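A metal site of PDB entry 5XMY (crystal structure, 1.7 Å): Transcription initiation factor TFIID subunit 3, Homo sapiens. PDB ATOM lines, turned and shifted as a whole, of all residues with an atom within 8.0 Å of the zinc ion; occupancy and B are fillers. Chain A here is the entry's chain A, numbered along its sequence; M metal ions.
The backbone carbonyl oxygen (O) of Pro 22 sits at hydrogen-bond distance from a ring nitrogen (NE2) of His 39.
N of Cys 16 is in hydrogen-bond range of O of Lys 21, at 2.9 Å.
The side-chain sulfur of Cys 16 lies close to the backbone NH of Gly 18.
The side-chain sulfur of Cys 19 lies close to the backbone NH of Lys 21, 3.6 Å away.
ND1 of His 39 is bound to the zinc ion (2.1 Å).
The zinc ion is bound by the side-chain sulfur (SG) of Cys 42 (2.3 Å).
SG of Cys 19 binds the zinc ion (2.3 Å).
The side-chain sulfur (SG) of Cys 16 binds the zinc ion.
The zinc ion has four donor atoms within binding distance.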
ATOM      1  N   ILE A  15      24.873  32.702  25.510  1.00  0.00           N
ATOM      2  CA  ILE A  15      25.821  31.642  25.185  1.00  0.00           C
ATOM      3  C   ILE A  15      26.352  31.055  26.487  1.00  0.00           C
ATOM      4  O   ILE A  15      26.720  31.815  27.393  1.00  0.00           O
ATOM      5  CB  ILE A  15      26.977  32.174  24.323  1.00  0.00           C
ATOM      6  CG1 ILE A  15      26.437  32.843  23.051  1.00  0.00           C
ATOM      7  CG2 ILE A  15      27.959  31.060  24.008  1.00  0.00           C
ATOM      8  CD1 ILE A  15      25.589  31.942  22.197  1.00  0.00           C
ATOM      9  N   CYS A  16      26.390  29.731  26.576  1.00  0.00           N
ATOM     10  CA  CYS A  16      26.933  29.030  27.739  1.00  0.00           C
ATOM     11  C   CYS A  16      28.456  29.112  27.762  1.00  0.00           C
ATOM     12  O   CYS A  16      29.104  28.668  26.800  1.00  0.00           O
ATOM     13  CB  CYS A  16      26.506  27.562  27.700  1.00  0.00           C
ATOM     14  SG  CYS A  16      27.211  26.509  29.002  1.00  0.00           S
ATOM     15  N   PRO A  17      29.073  29.661  28.814  1.00  0.00           N
ATOM     16  CA  PRO A  17      30.545  29.729  28.858  1.00  0.00           C
ATOM     17  C   PRO A  17      31.214  28.376  28.962  1.00  0.00           C
ATOM     18  O   PRO A  17      32.424  28.272  28.664  1.00  0.00           O
ATOM     19  CB  PRO A  17      30.819  30.555  30.126  1.00  0.00           C
ATOM     20  CG  PRO A  17      29.565  31.379  30.319  1.00  0.00           C
ATOM     21  CD  PRO A  17      28.476  30.402  29.933  1.00  0.00           C
ATOM     22  N   GLY A  18      30.489  27.343  29.367  1.00  0.00           N
ATOM     23  CA  GLY A  18      31.114  26.036  29.492  1.00  0.00           C
ATOM     24  C   GLY A  18      31.417  25.399  28.150  1.00  0.00           C
ATOM     25  O   GLY A  18      32.451  24.754  27.980  1.00  0.00           O
ATOM     26  N   CYS A  19      30.522  25.592  27.179  1.00  0.00           N
ATOM     27  CA  CYS A  19      30.643  24.948  25.871  1.00  0.00           C
ATOM     28  C   CYS A  19      30.646  25.913  24.693  1.00  0.00           C
ATOM     29  O   CYS A  19      30.806  25.468  23.542  1.00  0.00           O
ATOM     30  CB  CYS A  19      29.503  23.930  25.686  1.00  0.00           C
ATOM     31  SG  CYS A  19      27.828  24.653  25.640  1.00  0.00           S
ATOM     32  N   ASN A  20      30.482  27.216  24.937  1.00  0.00           N
ATOM     33  CA  ASN A  20      30.398  28.254  23.911  1.00  0.00           C
ATOM     34  C   ASN A  20      29.265  28.012  22.900  1.00  0.00           C
ATOM     35  O   ASN A  20      29.332  28.506  21.774  1.00  0.00           O
ATOM     36  CB  ASN A  20      31.732  28.422  23.168  1.00  0.00           C
ATOM     37  CG  ASN A  20      32.844  28.927  24.068  1.00  0.00           C
ATOM     38  OD1 ASN A  20      33.983  28.451  23.994  1.00  0.00           O
ATOM     39  ND2 ASN A  20      32.534  29.912  24.908  1.00  0.00           N
ATOM     40  N   LYS A  21      28.224  27.280  23.280  1.00  0.00           N
ATOM     41  CA  LYS A  21      27.037  27.037  22.480  1.00  0.00           C
ATOM     42  C   LYS A  21      25.837  27.818  23.033  1.00  0.00           C
ATOM     43  O   LYS A  21      25.753  28.053  24.244  1.00  0.00           O
ATOM     44  CB  LYS A  21      26.667  25.551  22.430  1.00  0.00           C
ATOM     45  CG  LYS A  21      27.719  24.646  21.802  1.00  0.00           C
ATOM     46  CD  LYS A  21      27.185  23.230  21.645  1.00  0.00           C
ATOM     47  CE  LYS A  21      28.194  22.320  20.958  1.00  0.00           C
ATOM     48  NZ  LYS A  21      27.607  20.990  20.662  1.00  0.00           N
ATOM     49  N   PRO A  22      24.875  28.181  22.193  1.00  0.00           N
ATOM     50  CA  PRO A  22      23.736  28.984  22.664  1.00  0.00           C
ATOM     51  C   PRO A  22      22.750  28.199  23.514  1.00  0.00           C
ATOM     52  O   PRO A  22      22.686  26.968  23.495  1.00  0.00           O
ATOM     53  CB  PRO A  22      23.069  29.447  21.356  1.00  0.00           C
ATOM     54  CG  PRO A  22      24.076  29.158  20.264  1.00  0.00           C
ATOM     55  CD  PRO A  22      24.836  27.979  20.725  1.00  0.00           C
ATOM     56  N   ASP A  23      21.976  28.959  24.277  1.00  0.00           N
ATOM     57  CA  ASP A  23      20.695  28.531  24.821  1.00  0.00           C
ATOM     58  C   ASP A  23      19.854  27.899  23.715  1.00  0.00           C
ATOM     59  O   ASP A  23      19.673  28.495  22.645  1.00  0.00           O
ATOM     60  CB  ASP A  23      19.994  29.753  25.389  1.00  0.00           C
ATOM     61  CG  ASP A  23      18.641  29.456  26.023  1.00  0.00           C
ATOM     62  OD1 ASP A  23      18.265  28.275  26.211  1.00  0.00           O
ATOM     63  OD2 ASP A  23      17.967  30.451  26.362  1.00  0.00           O
ATOM     64  N   SER A  26      16.882  23.894  26.357  1.00  0.00           N
ATOM     65  CA  SER A  26      17.210  22.937  27.407  1.00  0.00           C
ATOM     66  C   SER A  26      17.564  23.683  28.693  1.00  0.00           C
ATOM     67  O   SER A  26      17.856  24.885  28.667  1.00  0.00           O
ATOM     68  CB  SER A  26      18.357  22.043  26.956  1.00  0.00           C
ATOM     69  OG  SER A  26      19.534  22.781  26.753  1.00  0.00           O
ATOM     70  N   PRO A  27      17.506  23.007  29.840  1.00  0.00           N
ATOM     71  CA  PRO A  27      17.606  23.733  31.123  1.00  0.00           C
ATOM     72  C   PRO A  27      18.948  24.434  31.286  1.00  0.00           C
ATOM     73  O   PRO A  27      20.000  23.885  30.945  1.00  0.00           O
ATOM     74  CB  PRO A  27      17.401  22.631  32.166  1.00  0.00           C
ATOM     75  CG  PRO A  27      16.638  21.580  31.452  1.00  0.00           C
ATOM     76  CD  PRO A  27      17.201  21.576  30.069  1.00  0.00           C
ATOM     77  N   MET A  28      18.882  25.667  31.788  1.00  0.00           N
ATOM     78  CA  MET A  28      20.057  26.450  32.124  1.00  0.00           C
ATOM     79  C   MET A  28      19.921  26.956  33.554  1.00  0.00           C
ATOM     80  O   MET A  28      18.845  26.946  34.140  1.00  0.00           O
ATOM     81  CB  MET A  28      20.252  27.625  31.150  1.00  0.00           C
ATOM     82  CG  MET A  28      20.309  27.220  29.692  1.00  0.00           C
ATOM     83  SD  MET A  28      20.772  28.612  28.630  1.00  0.00           S
ATOM     84  CE  MET A  28      22.565  28.509  28.668  1.00  0.00           C
ATOM     85  N   TRP A  37      24.796  32.489  32.115  1.00  0.00           N
ATOM     86  CA  TRP A  37      23.897  31.342  32.146  1.00  0.00           C
ATOM     87  C   TRP A  37      24.557  30.124  31.539  1.00  0.00           C
ATOM     88  O   TRP A  37      25.209  30.212  30.482  1.00  0.00           O
ATOM     89  CB  TRP A  37      22.599  31.658  31.394  1.00  0.00           C
ATOM     90  CG  TRP A  37      21.679  32.537  32.179  1.00  0.00           C
ATOM     91  CD1 TRP A  37      21.760  33.889  32.307  1.00  0.00           C
ATOM     92  CD2 TRP A  37      20.556  32.121  32.970  1.00  0.00           C
ATOM     93  NE1 TRP A  37      20.738  34.348  33.129  1.00  0.00           N
ATOM     94  CE2 TRP A  37      19.988  33.277  33.535  1.00  0.00           C
ATOM     95  CE3 TRP A  37      19.972  30.877  33.223  1.00  0.00           C
ATOM     96  CZ2 TRP A  37      18.860  33.215  34.372  1.00  0.00           C
ATOM     97  CZ3 TRP A  37      18.845  30.825  34.031  1.00  0.00           C
ATOM     98  CH2 TRP A  37      18.308  31.987  34.595  1.00  0.00           C
ATOM     99  N   TYR A  38      24.399  28.982  32.201  1.00  0.00           N
ATOM    100  CA  TYR A  38      25.029  27.729  31.816  1.00  0.00           C
ATOM    101  C   TYR A  38      24.000  26.636  31.588  1.00  0.00           C
ATOM    102  O   TYR A  38      22.996  26.538  32.313  1.00  0.00           O
ATOM    103  CB  TYR A  38      26.015  27.204  32.866  1.00  0.00           C
ATOM    104  CG  TYR A  38      27.296  27.982  33.020  1.00  0.00           C
ATOM    105  CD1 TYR A  38      27.316  29.236  33.630  1.00  0.00           C
ATOM    106  CD2 TYR A  38      28.510  27.453  32.575  1.00  0.00           C
ATOM    107  CE1 TYR A  38      28.497  29.946  33.767  1.00  0.00           C
ATOM    108  CE2 TYR A  38      29.700  28.152  32.731  1.00  0.00           C
ATOM    109  CZ  TYR A  38      29.689  29.399  33.322  1.00  0.00           C
ATOM    110  OH  TYR A  38      30.858  30.101  33.459  1.00  0.00           O
ATOM    111  N   HIS A  39      24.281  25.764  30.618  1.00  0.00           N
ATOM    112  CA  HIS A  39      23.537  24.516  30.495  1.00  0.00           C
ATOM    113  C   HIS A  39      23.761  23.664  31.727  1.00  0.00           C
ATOM    114  O   HIS A  39      24.885  23.539  32.211  1.00  0.00           O
ATOM    115  CB  HIS A  39      23.972  23.713  29.260  1.00  0.00           C
ATOM    116  CG  HIS A  39      23.854  24.450  27.967  1.00  0.00           C
ATOM    117  ND1 HIS A  39      24.940  24.739  27.169  1.00  0.00           N
ATOM    118  CD2 HIS A  39      22.773  24.951  27.319  1.00  0.00           C
ATOM    119  CE1 HIS A  39      24.534  25.393  26.093  1.00  0.00           C
ATOM    120  NE2 HIS A  39      23.222  25.528  26.164  1.00  0.00           N
ATOM    121  N   TRP A  40      22.688  23.058  32.237  1.00  0.00           N
ATOM    122  CA  TRP A  40      22.836  22.175  33.400  1.00  0.00           C
ATOM    123  C   TRP A  40      23.931  21.129  33.222  1.00  0.00           C
ATOM    124  O   TRP A  40      24.807  21.039  34.102  1.00  0.00           O
ATOM    125  CB  TRP A  40      21.507  21.478  33.748  1.00  0.00           C
ATOM    126  CG  TRP A  40      20.459  22.332  34.396  1.00  0.00           C
ATOM    127  CD1 TRP A  40      20.474  23.703  34.556  1.00  0.00           C
ATOM    128  CD2 TRP A  40      19.236  21.876  34.959  1.00  0.00           C
ATOM    129  NE1 TRP A  40      19.309  24.107  35.191  1.00  0.00           N
ATOM    130  CE2 TRP A  40      18.542  23.006  35.447  1.00  0.00           C
ATOM    131  CE3 TRP A  40      18.647  20.611  35.103  1.00  0.00           C
ATOM    132  CZ2 TRP A  40      17.284  22.909  36.078  1.00  0.00           C
ATOM    133  CZ3 TRP A  40      17.400  20.522  35.724  1.00  0.00           C
ATOM    134  CH2 TRP A  40      16.736  21.658  36.191  1.00  0.00           C
ATOM    135  N   PRO A  41      23.955  20.309  32.167  1.00  0.00           N
ATOM    136  CA  PRO A  41      25.026  19.297  32.090  1.00  0.00           C
ATOM    137  C   PRO A  41      26.412  19.899  32.072  1.00  0.00           C
ATOM    138  O   PRO A  41      27.354  19.283  32.594  1.00  0.00           O
ATOM    139  CB  PRO A  41      24.709  18.537  30.792  1.00  0.00           C
ATOM    140  CG  PRO A  41      23.772  19.402  30.038  1.00  0.00           C
ATOM    141  CD  PRO A  41      22.995  20.175  31.051  1.00  0.00           C
ATOM    142  N   CYS A  42      26.560  21.105  31.529  1.00  0.00           N
ATOM    143  CA  CYS A  42      27.860  21.757  31.443  1.00  0.00           C
ATOM    144  C   CYS A  42      28.439  22.102  32.807  1.00  0.00           C
ATOM    145  O   CYS A  42      29.651  22.345  32.906  1.00  0.00           O
ATOM    146  CB  CYS A  42      27.734  23.003  30.566  1.00  0.00           C
ATOM    147  SG  CYS A  42      27.351  22.590  28.848  1.00  0.00           S
ATOM    148  N   VAL A  43      27.620  22.135  33.857  1.00  0.00           N
ATOM    149  CA  VAL A  43      28.094  22.453  35.193  1.00  0.00           C
ATOM    150  C   VAL A  43      27.666  21.358  36.162  1.00  0.00           C
ATOM    151  O   VAL A  43      27.630  21.567  37.382  1.00  0.00           O
ATOM    152  CB  VAL A  43      27.603  23.840  35.655  1.00  0.00           C
ATOM    153  CG1 VAL A  43      28.314  24.911  34.869  1.00  0.00           C
ATOM    154  CG2 VAL A  43      26.094  23.976  35.480  1.00  0.00           C
HETATM  155 ZN    ZN M   1      26.959  24.573  27.762  1.00  0.00          ZN
